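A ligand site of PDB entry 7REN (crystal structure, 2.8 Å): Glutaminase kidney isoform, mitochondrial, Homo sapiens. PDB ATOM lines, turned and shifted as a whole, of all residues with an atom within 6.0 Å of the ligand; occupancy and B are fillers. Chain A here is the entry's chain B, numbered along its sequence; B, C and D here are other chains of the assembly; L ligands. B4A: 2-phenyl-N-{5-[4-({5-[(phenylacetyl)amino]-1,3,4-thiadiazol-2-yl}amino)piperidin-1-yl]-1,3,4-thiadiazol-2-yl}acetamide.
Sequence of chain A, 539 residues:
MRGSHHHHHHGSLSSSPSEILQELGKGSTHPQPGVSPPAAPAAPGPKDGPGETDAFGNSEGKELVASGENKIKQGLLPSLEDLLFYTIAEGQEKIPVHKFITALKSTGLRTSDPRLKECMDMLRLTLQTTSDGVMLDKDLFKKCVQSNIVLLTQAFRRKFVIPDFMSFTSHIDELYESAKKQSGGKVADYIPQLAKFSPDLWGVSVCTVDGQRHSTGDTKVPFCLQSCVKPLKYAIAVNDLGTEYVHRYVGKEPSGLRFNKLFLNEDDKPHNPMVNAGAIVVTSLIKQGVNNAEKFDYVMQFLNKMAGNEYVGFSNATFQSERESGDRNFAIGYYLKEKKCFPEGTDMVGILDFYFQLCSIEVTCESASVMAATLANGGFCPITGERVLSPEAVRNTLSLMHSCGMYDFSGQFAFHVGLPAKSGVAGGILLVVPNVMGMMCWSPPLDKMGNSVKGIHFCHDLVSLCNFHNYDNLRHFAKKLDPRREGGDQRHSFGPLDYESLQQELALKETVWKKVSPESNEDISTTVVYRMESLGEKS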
ATOM      1  N   ARG A 258      -7.339   6.945 -13.045  1.00  0.00           N
ATOM      2  CA  ARG A 258      -8.116   5.981 -13.805  1.00  0.00           C
ATOM      3  C   ARG A 258      -8.887   5.015 -12.901  1.00  0.00           C
ATOM      4  O   ARG A 258     -10.019   4.640 -13.248  1.00  0.00           O
ATOM      5  CB  ARG A 258      -7.155   5.204 -14.709  1.00  0.00           C
ATOM      6  CG  ARG A 258      -7.795   4.239 -15.643  1.00  0.00           C
ATOM      7  CD  ARG A 258      -8.985   4.810 -16.328  1.00  0.00           C
ATOM      8  NE  ARG A 258      -9.928   3.758 -16.675  1.00  0.00           N
ATOM      9  CZ  ARG A 258     -10.866   3.914 -17.600  1.00  0.00           C
ATOM     10  NH1 ARG A 258     -10.944   5.051 -18.259  1.00  0.00           N
ATOM     11  NH2 ARG A 258     -11.688   2.913 -17.869  1.00  0.00           N
ATOM     12  N   PHE A 259      -8.328   4.614 -11.762  1.00  0.00           N
ATOM     13  CA  PHE A 259      -8.994   3.673 -10.859  1.00  0.00           C
ATOM     14  C   PHE A 259      -9.822   4.367  -9.782  1.00  0.00           C
ATOM     15  O   PHE A 259     -10.139   3.747  -8.767  1.00  0.00           O
ATOM     16  CB  PHE A 259      -7.954   2.735 -10.222  1.00  0.00           C
ATOM     17  CG  PHE A 259      -7.225   1.885 -11.227  1.00  0.00           C
ATOM     18  CD1 PHE A 259      -6.053   1.216 -10.890  1.00  0.00           C
ATOM     19  CD2 PHE A 259      -7.716   1.755 -12.524  1.00  0.00           C
ATOM     20  CE1 PHE A 259      -5.376   0.454 -11.827  1.00  0.00           C
ATOM     21  CE2 PHE A 259      -7.055   0.998 -13.467  1.00  0.00           C
ATOM     22  CZ  PHE A 259      -5.890   0.340 -13.118  1.00  0.00           C
ATOM     23  N   LYS A 261     -12.851   4.938  -9.776  1.00  0.00           N
ATOM     24  CA  LYS A 261     -14.123   4.269  -9.578  1.00  0.00           C
ATOM     25  C   LYS A 261     -14.040   2.772  -9.871  1.00  0.00           C
ATOM     26  O   LYS A 261     -14.996   2.158 -10.354  1.00  0.00           O
ATOM     27  CB  LYS A 261     -15.237   4.967 -10.373  1.00  0.00           C
ATOM     28  CG  LYS A 261     -14.825   5.671 -11.639  1.00  0.00           C
ATOM     29  CD  LYS A 261     -16.072   6.225 -12.357  1.00  0.00           C
ATOM     30  CE  LYS A 261     -15.932   6.225 -13.883  1.00  0.00           C
ATOM     31  NZ  LYS A 261     -16.866   7.195 -14.537  1.00  0.00           N
ATOM     32  N   LEU A 262     -12.918   2.157  -9.592  1.00  0.00           N
ATOM     33  CA  LEU A 262     -12.930   0.754  -9.208  1.00  0.00           C
ATOM     34  C   LEU A 262     -12.837   0.646  -7.689  1.00  0.00           C
ATOM     35  O   LEU A 262     -12.273   1.524  -7.023  1.00  0.00           O
ATOM     36  CB  LEU A 262     -11.775  -0.014  -9.832  1.00  0.00           C
ATOM     37  CG  LEU A 262     -11.832  -0.291 -11.330  1.00  0.00           C
ATOM     38  CD1 LEU A 262     -11.422   0.946 -12.150  1.00  0.00           C
ATOM     39  CD2 LEU A 262     -10.932  -1.479 -11.619  1.00  0.00           C
ATOM     40  N   PHE A 263     -13.394  -0.428  -7.134  1.00  0.00           N
ATOM     41  CA  PHE A 263     -13.512  -0.516  -5.683  1.00  0.00           C
ATOM     42  C   PHE A 263     -12.361  -1.315  -5.068  1.00  0.00           C
ATOM     43  O   PHE A 263     -11.724  -0.856  -4.108  1.00  0.00           O
ATOM     44  CB  PHE A 263     -14.857  -1.151  -5.265  1.00  0.00           C
ATOM     45  CG  PHE A 263     -16.103  -0.419  -5.802  1.00  0.00           C
ATOM     46  CD1 PHE A 263     -16.069   0.921  -6.169  1.00  0.00           C
ATOM     47  CD2 PHE A 263     -17.308  -1.105  -5.918  1.00  0.00           C
ATOM     48  CE1 PHE A 263     -17.229   1.565  -6.654  1.00  0.00           C
ATOM     49  CE2 PHE A 263     -18.474  -0.455  -6.376  1.00  0.00           C
ATOM     50  CZ  PHE A 263     -18.426   0.874  -6.759  1.00  0.00           C
ATOM     51  N   LEU A 264     -12.079  -2.476  -5.619  1.00  0.00           N
ATOM     52  CA  LEU A 264     -11.066  -3.385  -5.120  1.00  0.00           C
ATOM     53  C   LEU A 264      -9.833  -3.336  -6.002  1.00  0.00           C
ATOM     54  O   LEU A 264      -9.833  -2.727  -7.068  1.00  0.00           O
ATOM     55  CB  LEU A 264     -11.600  -4.808  -5.049  1.00  0.00           C
ATOM     56  CG  LEU A 264     -12.818  -4.881  -4.151  1.00  0.00           C
ATOM     57  CD1 LEU A 264     -13.059  -6.321  -3.823  1.00  0.00           C
ATOM     58  CD2 LEU A 264     -12.502  -4.084  -2.909  1.00  0.00           C
ATOM     59  N   ASN A 265      -8.778  -3.963  -5.523  1.00  0.00           N
ATOM     60  CA  ASN A 265      -7.531  -4.077  -6.261  1.00  0.00           C
ATOM     61  C   ASN A 265      -7.327  -5.547  -6.604  1.00  0.00           C
ATOM     62  O   ASN A 265      -8.169  -6.404  -6.305  1.00  0.00           O
ATOM     63  CB  ASN A 265      -6.356  -3.470  -5.466  1.00  0.00           C
ATOM     64  CG  ASN A 265      -5.952  -4.290  -4.234  1.00  0.00           C
ATOM     65  OD1 ASN A 265      -6.221  -5.482  -4.121  1.00  0.00           O
ATOM     66  ND2 ASN A 265      -5.282  -3.628  -3.289  1.00  0.00           N
ATOM     67  N   GLU A 266      -6.169  -5.829  -7.206  1.00  0.00           N
ATOM     68  CA  GLU A 266      -5.894  -7.155  -7.750  1.00  0.00           C
ATOM     69  C   GLU A 266      -6.037  -8.249  -6.694  1.00  0.00           C
ATOM     70  O   GLU A 266      -6.535  -9.345  -6.993  1.00  0.00           O
ATOM     71  CB  GLU A 266      -4.506  -7.169  -8.370  1.00  0.00           C
ATOM     72  CG  GLU A 266      -4.211  -5.879  -9.130  1.00  0.00           C
ATOM     73  CD  GLU A 266      -2.862  -5.881  -9.820  1.00  0.00           C
ATOM     74  OE1 GLU A 266      -2.556  -4.888 -10.523  1.00  0.00           O
ATOM     75  OE2 GLU A 266      -2.099  -6.866  -9.662  1.00  0.00           O
ATOM     76  N   ASP A 267      -5.638  -7.978  -5.445  1.00  0.00           N
ATOM     77  CA  ASP A 267      -5.774  -8.929  -4.348  1.00  0.00           C
ATOM     78  C   ASP A 267      -7.141  -8.865  -3.689  1.00  0.00           C
ATOM     79  O   ASP A 267      -7.307  -9.421  -2.583  1.00  0.00           O
ATOM     80  CB  ASP A 267      -4.671  -8.725  -3.303  1.00  0.00           C
ATOM     81  CG  ASP A 267      -3.320  -9.225  -3.781  1.00  0.00           C
ATOM     82  OD1 ASP A 267      -3.098 -10.454  -3.729  1.00  0.00           O
ATOM     83  OD2 ASP A 267      -2.483  -8.403  -4.200  1.00  0.00           O
ATOM     84  N   ASP A 268      -8.098  -8.190  -4.316  1.00  0.00           N
ATOM     85  CA  ASP A 268      -9.511  -8.169  -3.925  1.00  0.00           C
ATOM     86  C   ASP A 268      -9.746  -7.465  -2.576  1.00  0.00           C
ATOM     87  O   ASP A 268     -10.789  -7.659  -1.946  1.00  0.00           O
ATOM     88  CB  ASP A 268     -10.104  -9.581  -3.900  1.00  0.00           C
ATOM     89  CG  ASP A 268     -10.444 -10.087  -5.291  1.00  0.00           C
ATOM     90  OD1 ASP A 268     -10.290  -9.302  -6.257  1.00  0.00           O
ATOM     91  OD2 ASP A 268     -10.873 -11.256  -5.419  1.00  0.00           O
ATOM     92  N   HIS A 271      -8.292  -0.392  -2.289  1.00  0.00           N
ATOM     93  CA  HIS A 271      -6.935   0.089  -2.565  1.00  0.00           C
ATOM     94  C   HIS A 271      -6.264   0.628  -1.308  1.00  0.00           C
ATOM     95  O   HIS A 271      -5.155   0.221  -0.968  1.00  0.00           O
ATOM     96  CB  HIS A 271      -6.965   1.135  -3.668  1.00  0.00           C
ATOM     97  CG  HIS A 271      -7.456   0.602  -4.964  1.00  0.00           C
ATOM     98  ND1 HIS A 271      -6.679  -0.192  -5.783  1.00  0.00           N
ATOM     99  CD2 HIS A 271      -8.661   0.697  -5.579  1.00  0.00           C
ATOM    100  CE1 HIS A 271      -7.377  -0.546  -6.844  1.00  0.00           C
ATOM    101  NE2 HIS A 271      -8.579  -0.010  -6.743  1.00  0.00           N
ATOM    102  N   TYR A 335     -21.112  -4.941  -2.972  1.00  0.00           N
ATOM    103  CA  TYR A 335     -19.987  -5.513  -3.720  1.00  0.00           C
ATOM    104  C   TYR A 335     -18.929  -6.071  -2.780  1.00  0.00           C
ATOM    105  O   TYR A 335     -18.329  -7.126  -3.046  1.00  0.00           O
ATOM    106  CB  TYR A 335     -19.371  -4.466  -4.654  1.00  0.00           C
ATOM    107  CG  TYR A 335     -18.404  -5.046  -5.682  1.00  0.00           C
ATOM    108  CD1 TYR A 335     -18.865  -5.827  -6.726  1.00  0.00           C
ATOM    109  CD2 TYR A 335     -17.034  -4.815  -5.605  1.00  0.00           C
ATOM    110  CE1 TYR A 335     -18.001  -6.374  -7.666  1.00  0.00           C
ATOM    111  CE2 TYR A 335     -16.157  -5.357  -6.544  1.00  0.00           C
ATOM    112  CZ  TYR A 335     -16.646  -6.133  -7.573  1.00  0.00           C
ATOM    113  OH  TYR A 335     -15.790  -6.675  -8.523  1.00  0.00           O
ATOM    114  N   LYS A 339     -17.721 -10.225  -2.458  1.00  0.00           N
ATOM    115  CA  LYS A 339     -16.345 -10.687  -2.538  1.00  0.00           C
ATOM    116  C   LYS A 339     -15.798 -11.166  -1.189  1.00  0.00           C
ATOM    117  O   LYS A 339     -14.625 -11.553  -1.140  1.00  0.00           O
ATOM    118  CB  LYS A 339     -15.487  -9.564  -3.126  1.00  0.00           C
ATOM    119  CG  LYS A 339     -15.908  -9.181  -4.546  1.00  0.00           C
ATOM    120  CD  LYS A 339     -15.701 -10.368  -5.547  1.00  0.00           C
ATOM    121  CE  LYS A 339     -15.763  -9.928  -7.003  1.00  0.00           C
ATOM    122  NZ  LYS A 339     -16.010 -11.090  -7.909  1.00  0.00           N
ATOM    123  N   ARG B 258     -11.596  -7.475 -20.709  1.00  0.00           N
ATOM    124  CA  ARG B 258     -11.201  -6.834 -19.455  1.00  0.00           C
ATOM    125  C   ARG B 258     -12.380  -6.154 -18.763  1.00  0.00           C
ATOM    126  O   ARG B 258     -12.294  -5.840 -17.567  1.00  0.00           O
ATOM    127  CB  ARG B 258     -10.056  -5.837 -19.730  1.00  0.00           C
ATOM    128  CG  ARG B 258      -9.931  -4.595 -18.823  1.00  0.00           C
ATOM    129  CD  ARG B 258      -9.351  -4.886 -17.419  1.00  0.00           C
ATOM    130  NE  ARG B 258      -9.232  -3.656 -16.629  1.00  0.00           N
ATOM    131  CZ  ARG B 258     -10.222  -3.123 -15.908  1.00  0.00           C
ATOM    132  NH1 ARG B 258     -11.403  -3.703 -15.861  1.00  0.00           N
ATOM    133  NH2 ARG B 258     -10.019  -2.004 -15.233  1.00  0.00           N
ATOM    134  N   PHE B 259     -13.502  -5.999 -19.458  1.00  0.00           N
ATOM    135  CA  PHE B 259     -14.653  -5.257 -18.940  1.00  0.00           C
ATOM    136  C   PHE B 259     -15.807  -6.182 -18.541  1.00  0.00           C
ATOM    137  O   PHE B 259     -16.962  -5.750 -18.483  1.00  0.00           O
ATOM    138  CB  PHE B 259     -15.097  -4.223 -19.969  1.00  0.00           C
ATOM    139  CG  PHE B 259     -14.066  -3.124 -20.209  1.00  0.00           C
ATOM    140  CD1 PHE B 259     -13.083  -2.859 -19.270  1.00  0.00           C
ATOM    141  CD2 PHE B 259     -14.084  -2.363 -21.374  1.00  0.00           C
ATOM    142  CE1 PHE B 259     -12.129  -1.854 -19.481  1.00  0.00           C
ATOM    143  CE2 PHE B 259     -13.136  -1.375 -21.598  1.00  0.00           C
ATOM    144  CZ  PHE B 259     -12.165  -1.108 -20.640  1.00  0.00           C
ATOM    145  N   LYS B 261     -16.016  -6.723 -15.609  1.00  0.00           N
ATOM    146  CA  LYS B 261     -16.192  -6.207 -14.269  1.00  0.00           C
ATOM    147  C   LYS B 261     -16.704  -4.766 -14.216  1.00  0.00           C
ATOM    148  O   LYS B 261     -16.986  -4.293 -13.108  1.00  0.00           O
ATOM    149  CB  LYS B 261     -14.865  -6.316 -13.533  1.00  0.00           C
ATOM    150  CG  LYS B 261     -14.281  -7.737 -13.602  1.00  0.00           C
ATOM    151  CD  LYS B 261     -12.886  -7.798 -13.059  1.00  0.00           C
ATOM    152  CE  LYS B 261     -12.131  -6.528 -13.411  1.00  0.00           C
ATOM    153  NZ  LYS B 261     -11.913  -6.348 -14.892  1.00  0.00           N
ATOM    154  N   LEU B 262     -16.852  -4.069 -15.334  1.00  0.00           N
ATOM    155  CA  LEU B 262     -17.520  -2.779 -15.327  1.00  0.00           C
ATOM    156  C   LEU B 262     -19.024  -2.918 -15.542  1.00  0.00           C
ATOM    157  O   LEU B 262     -19.525  -3.984 -15.891  1.00  0.00           O
ATOM    158  CB  LEU B 262     -16.955  -1.862 -16.397  1.00  0.00           C
ATOM    159  CG  LEU B 262     -15.779  -1.091 -15.846  1.00  0.00           C
ATOM    160  CD1 LEU B 262     -14.511  -1.888 -16.068  1.00  0.00           C
ATOM    161  CD2 LEU B 262     -15.728   0.266 -16.537  1.00  0.00           C
ATOM    162  N   PHE B 263     -19.757  -1.820 -15.315  1.00  0.00           N
ATOM    163  CA  PHE B 263     -21.211  -1.851 -15.434  1.00  0.00           C
ATOM    164  C   PHE B 263     -21.746  -0.937 -16.515  1.00  0.00           C
ATOM    165  O   PHE B 263     -22.759  -1.259 -17.140  1.00  0.00           O
ATOM    166  CB  PHE B 263     -21.903  -1.481 -14.110  1.00  0.00           C
ATOM    167  CG  PHE B 263     -21.570  -2.386 -12.946  1.00  0.00           C
ATOM    168  CD1 PHE B 263     -21.022  -3.658 -13.140  1.00  0.00           C
ATOM    169  CD2 PHE B 263     -21.787  -1.969 -11.635  1.00  0.00           C
ATOM    170  CE1 PHE B 263     -20.700  -4.486 -12.082  1.00  0.00           C
ATOM    171  CE2 PHE B 263     -21.477  -2.796 -10.557  1.00  0.00           C
ATOM    172  CZ  PHE B 263     -20.931  -4.067 -10.789  1.00  0.00           C
ATOM    173  N   LEU B 264     -21.083   0.181 -16.750  1.00  0.00           N
ATOM    174  CA  LEU B 264     -21.527   1.211 -17.675  1.00  0.00           C
ATOM    175  C   LEU B 264     -20.458   1.498 -18.722  1.00  0.00           C
ATOM    176  O   LEU B 264     -19.267   1.541 -18.431  1.00  0.00           O
ATOM    177  CB  LEU B 264     -21.830   2.510 -16.948  1.00  0.00           C
ATOM    178  CG  LEU B 264     -22.863   2.275 -15.872  1.00  0.00           C
ATOM    179  CD1 LEU B 264     -23.280   3.625 -15.263  1.00  0.00           C
ATOM    180  CD2 LEU B 264     -23.990   1.552 -16.553  1.00  0.00           C
ATOM    181  N   ASN B 265     -20.920   1.738 -19.934  1.00  0.00           N
ATOM    182  CA  ASN B 265     -20.045   2.283 -20.956  1.00  0.00           C
ATOM    183  C   ASN B 265     -19.817   3.779 -20.693  1.00  0.00           C
ATOM    184  O   ASN B 265     -20.322   4.357 -19.724  1.00  0.00           O
ATOM    185  CB  ASN B 265     -20.633   1.965 -22.345  1.00  0.00           C
ATOM    186  CG  ASN B 265     -21.835   2.839 -22.735  1.00  0.00           C
ATOM    187  OD1 ASN B 265     -22.217   3.770 -22.025  1.00  0.00           O
ATOM    188  ND2 ASN B 265     -22.402   2.553 -23.911  1.00  0.00           N
ATOM    189  N   GLU B 266     -19.020   4.403 -21.564  1.00  0.00           N
ATOM    190  CA  GLU B 266     -18.570   5.784 -21.359  1.00  0.00           C
ATOM    191  C   GLU B 266     -19.730   6.778 -21.311  1.00  0.00           C
ATOM    192  O   GLU B 266     -19.575   7.872 -20.747  1.00  0.00           O
ATOM    193  CB  GLU B 266     -17.610   6.176 -22.489  1.00  0.00           C
ATOM    194  CG  GLU B 266     -16.265   5.427 -22.464  1.00  0.00           C
ATOM    195  CD  GLU B 266     -16.296   4.088 -23.205  1.00  0.00           C
ATOM    196  OE1 GLU B 266     -15.247   3.720 -23.788  1.00  0.00           O
ATOM    197  OE2 GLU B 266     -17.333   3.391 -23.205  1.00  0.00           O
ATOM    198  N   ASP B 268     -22.504   6.393 -19.700  1.00  0.00           N
ATOM    199  CA  ASP B 268     -23.286   6.111 -18.504  1.00  0.00           C
ATOM    200  C   ASP B 268     -24.457   5.180 -18.766  1.00  0.00           C
ATOM    201  O   ASP B 268     -25.456   5.210 -18.042  1.00  0.00           O
ATOM    202  CB  ASP B 268     -23.790   7.410 -17.854  1.00  0.00           C
ATOM    203  CG  ASP B 268     -22.738   8.069 -16.994  1.00  0.00           C
ATOM    204  OD1 ASP B 268     -21.711   7.408 -16.685  1.00  0.00           O
ATOM    205  OD2 ASP B 268     -22.948   9.247 -16.636  1.00  0.00           O
ATOM    206  N   ARG B 328     -24.289  -9.501  -5.541  1.00  0.00           N
ATOM    207  CA  ARG B 328     -23.708  -8.830  -6.694  1.00  0.00           C
ATOM    208  C   ARG B 328     -24.745  -7.994  -7.437  1.00  0.00           C
ATOM    209  O   ARG B 328     -24.425  -6.916  -7.960  1.00  0.00           O
ATOM    210  CB  ARG B 328     -23.084  -9.851  -7.641  1.00  0.00           C
ATOM    211  CG  ARG B 328     -22.331  -9.166  -8.756  1.00  0.00           C
ATOM    212  CD  ARG B 328     -22.227  -9.983 -10.034  1.00  0.00           C
ATOM    213  NE  ARG B 328     -21.641  -9.193 -11.120  1.00  0.00           N
ATOM    214  CZ  ARG B 328     -20.370  -8.782 -11.182  1.00  0.00           C
ATOM    215  NH1 ARG B 328     -19.494  -9.091 -10.221  1.00  0.00           N
ATOM    216  NH2 ARG B 328     -19.940  -8.066 -12.224  1.00  0.00           N
ATOM    217  N   TYR B 335     -25.851   1.095  -8.114  1.00  0.00           N
ATOM    218  CA  TYR B 335     -25.007   1.875  -9.025  1.00  0.00           C
ATOM    219  C   TYR B 335     -25.828   2.495 -10.156  1.00  0.00           C
ATOM    220  O   TYR B 335     -25.588   3.647 -10.550  1.00  0.00           O
ATOM    221  CB  TYR B 335     -23.863   1.039  -9.609  1.00  0.00           C
ATOM    222  CG  TYR B 335     -22.795   1.913 -10.248  1.00  0.00           C
ATOM    223  CD1 TYR B 335     -21.681   2.315  -9.533  1.00  0.00           C
ATOM    224  CD2 TYR B 335     -22.931   2.395 -11.537  1.00  0.00           C
ATOM    225  CE1 TYR B 335     -20.710   3.153 -10.107  1.00  0.00           C
ATOM    226  CE2 TYR B 335     -21.962   3.242 -12.114  1.00  0.00           C
ATOM    227  CZ  TYR B 335     -20.860   3.610 -11.388  1.00  0.00           C
ATOM    228  OH  TYR B 335     -19.908   4.448 -11.937  1.00  0.00           O
ATOM    229  N   ARG C 258     -13.009   1.263 -25.338  1.00  0.00           N
ATOM    230  CA  ARG C 258     -11.937   1.843 -24.555  1.00  0.00           C
ATOM    231  C   ARG C 258     -10.562   1.404 -25.039  1.00  0.00           C
ATOM    232  O   ARG C 258      -9.593   2.139 -24.812  1.00  0.00           O
ATOM    233  CB  ARG C 258     -12.051   1.442 -23.097  1.00  0.00           C
ATOM    234  CG  ARG C 258     -12.921   2.323 -22.286  1.00  0.00           C
ATOM    235  CD  ARG C 258     -12.348   2.482 -20.901  1.00  0.00           C
ATOM    236  NE  ARG C 258     -11.211   3.399 -20.815  1.00  0.00           N
ATOM    237  CZ  ARG C 258      -9.974   3.051 -20.455  1.00  0.00           C
ATOM    238  NH1 ARG C 258      -9.692   1.792 -20.146  1.00  0.00           N
ATOM    239  NH2 ARG C 258      -9.015   3.966 -20.397  1.00  0.00           N
ATOM    240  N   ARG D 258      -1.469  -1.655 -12.017  1.00  0.00           N
ATOM    241  CA  ARG D 258      -1.697  -2.169 -13.373  1.00  0.00           C
ATOM    242  C   ARG D 258      -2.004  -1.024 -14.324  1.00  0.00           C
ATOM    243  O   ARG D 258      -2.872  -1.115 -15.201  1.00  0.00           O
ATOM    244  CB  ARG D 258      -2.791  -3.235 -13.376  1.00  0.00           C
ATOM    245  CG  ARG D 258      -2.611  -4.342 -14.450  1.00  0.00           C
ATOM    246  CD  ARG D 258      -1.152  -4.835 -14.630  1.00  0.00           C
ATOM    247  NE  ARG D 258      -0.354  -4.837 -13.398  1.00  0.00           N
ATOM    248  CZ  ARG D 258       0.956  -5.086 -13.335  1.00  0.00           C
ATOM    249  NH1 ARG D 258       1.633  -5.350 -14.446  1.00  0.00           N
ATOM    250  NH2 ARG D 258       1.574  -5.055 -12.159  1.00  0.00           N
HETATM  251  N12 B4A L   1     -18.610   2.929 -14.950  1.00  0.00           N
HETATM  252  C13 B4A L   1     -17.543   3.470 -15.734  1.00  0.00           C
HETATM  253  C15 B4A L   1     -16.562   4.656 -17.752  1.00  0.00           C
HETATM  254  C17 B4A L   1     -15.110   6.314 -18.712  1.00  0.00           C
HETATM  255  C20 B4A L   1     -15.712   3.655 -18.213  1.00  0.00           C
HETATM  256  C26 B4A L   1     -12.188  -4.688  -9.903  1.00  0.00           C
HETATM  257  C28 B4A L   1     -10.772  -6.787  -9.647  1.00  0.00           C
HETATM  258  C01 B4A L   1     -17.857  -2.822 -10.568  1.00  0.00           C
HETATM  259  C02 B4A L   1     -16.775  -3.613  -9.838  1.00  0.00           C
HETATM  260  N03 B4A L   1     -15.535  -2.800  -9.944  1.00  0.00           N
HETATM  261  C04 B4A L   1     -15.624  -1.489  -9.242  1.00  0.00           C
HETATM  262  C05 B4A L   1     -17.012  -0.867  -9.319  1.00  0.00           C
HETATM  263  C06 B4A L   1     -17.710  -1.330 -10.545  1.00  0.00           C
HETATM  264  N07 B4A L   1     -16.921  -0.840 -11.703  1.00  0.00           N
HETATM  265  C08 B4A L   1     -17.362   0.427 -12.273  1.00  0.00           C
HETATM  266  N09 B4A L   1     -17.505   1.579 -11.525  1.00  0.00           N
HETATM  267  N10 B4A L   1     -17.999   2.727 -12.514  1.00  0.00           N
HETATM  268  C11 B4A L   1     -18.165   2.192 -13.783  1.00  0.00           C
HETATM  269  C14 B4A L   1     -17.834   4.288 -16.998  1.00  0.00           C
HETATM  270  C16 B4A L   1     -16.261   5.986 -18.002  1.00  0.00           C
HETATM  271  C18 B4A L   1     -14.261   5.313 -19.173  1.00  0.00           C
HETATM  272  C19 B4A L   1     -14.557   3.987 -18.915  1.00  0.00           C
HETATM  273  O21 B4A L   1     -16.436   3.277 -15.368  1.00  0.00           O
HETATM  274  S22 B4A L   1     -17.767   0.727 -13.741  1.00  0.00           S
HETATM  275  C23 B4A L   1     -14.298  -3.444  -9.596  1.00  0.00           C
HETATM  276  N24 B4A L   1     -13.636  -3.506  -8.377  1.00  0.00           N
HETATM  277  N25 B4A L   1     -12.262  -4.314  -8.571  1.00  0.00           N
HETATM  278  N27 B4A L   1     -10.919  -5.361  -9.866  1.00  0.00           N
HETATM  279  C29 B4A L   1      -9.338  -7.331  -9.699  1.00  0.00           C
HETATM  280  C30 B4A L   1      -8.740  -6.915 -11.059  1.00  0.00           C
HETATM  281  C31 B4A L   1      -8.208  -5.634 -11.252  1.00  0.00           C
HETATM  282  C32 B4A L   1      -7.680  -5.272 -12.479  1.00  0.00           C
HETATM  283  C33 B4A L   1      -7.685  -6.184 -13.529  1.00  0.00           C
HETATM  284  C34 B4A L   1      -8.209  -7.458 -13.358  1.00  0.00           C
HETATM  285  C35 B4A L   1      -8.728  -7.825 -12.121  1.00  0.00           C
HETATM  286  O36 B4A L   1     -11.716  -7.481  -9.426  1.00  0.00           O
HETATM  287  S37 B4A L   1     -13.434  -4.163 -10.608  1.00  0.00           S
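The side-chain hydroxyl (OH) of Tyr 335 of chain B sits at hydrogen-bond distance from a nitrogen (N10) of the ligand (2.6 Å).
The backbone NH (N) of Phe 263 of chain A sits close to a nitrogen (N24) of the ligand (3.3 Å).
A nitrogen (N24) of the ligand sits at hydrogen-bond distance from the backbone NH (N) of Leu 264 of chain A, 3.3 Å away.
N of Phe 263 of chain B lies close to S22 of the ligand (3.6 Å).
NZ of Lys 261 of chain B lies within hydrogen-bond range of O of Arg 258 of chain B.
The backbone carbonyl oxygen (O) of Leu 264 of chain A lies within hydrogen-bond range of a ring nitrogen (NE2) of His 271 (3.0 Å).
The side-chain amide oxygen (OD1) of Asn 265 of chain A lies within hydrogen-bond range of the backbone NH (N) of Asp 268 of chain A, at 3.3 Å.
The side-chain amide oxygen (OD1) of Asn 265 of chain A lies within hydrogen-bond range of the backbone NH (N) of Asp 267, at 2.9 Å.
The side-chain carboxylate of Glu 266 of chain A is in salt-bridge range of the guanidinium group of Arg 258 of chain D, 3.6 Å away.
N09 of the ligand sits close to O of Lys 261 of chain A (2.8 Å).
Residues that only touch the ligand: Arg 258 of chain A (3.2 Å), Leu 262 of chain A (3.5 Å), Asn 265 of chain A (3.7 Å), Glu 266 of chain A (3.96 Å), Asp 268 of chain A (3.9 Å), Tyr 335 of chain A (3.4 Å), Lys 261 of chain B (3.1 Å), Leu 262 of chain B (3.3 Å), Leu 264 of chain B (3.4 Å), Asn 265 of chain B (3.7 Å), Glu 266 of chain B (3.9 Å) and Arg 258 of chain C (3.3 Å).
Hydrophobic or aromatic side chains that line the ligand: Leu 262 of chain A, Phe 263 of chain A, Leu 264 of chain A, Tyr 335 of chain A, Leu 262 of chain B, Phe 263 of chain B, Leu 264 of chain B and Tyr 335 of chain B.
Of the 26 residues printed, 17 come within 4 Å of the ligand.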
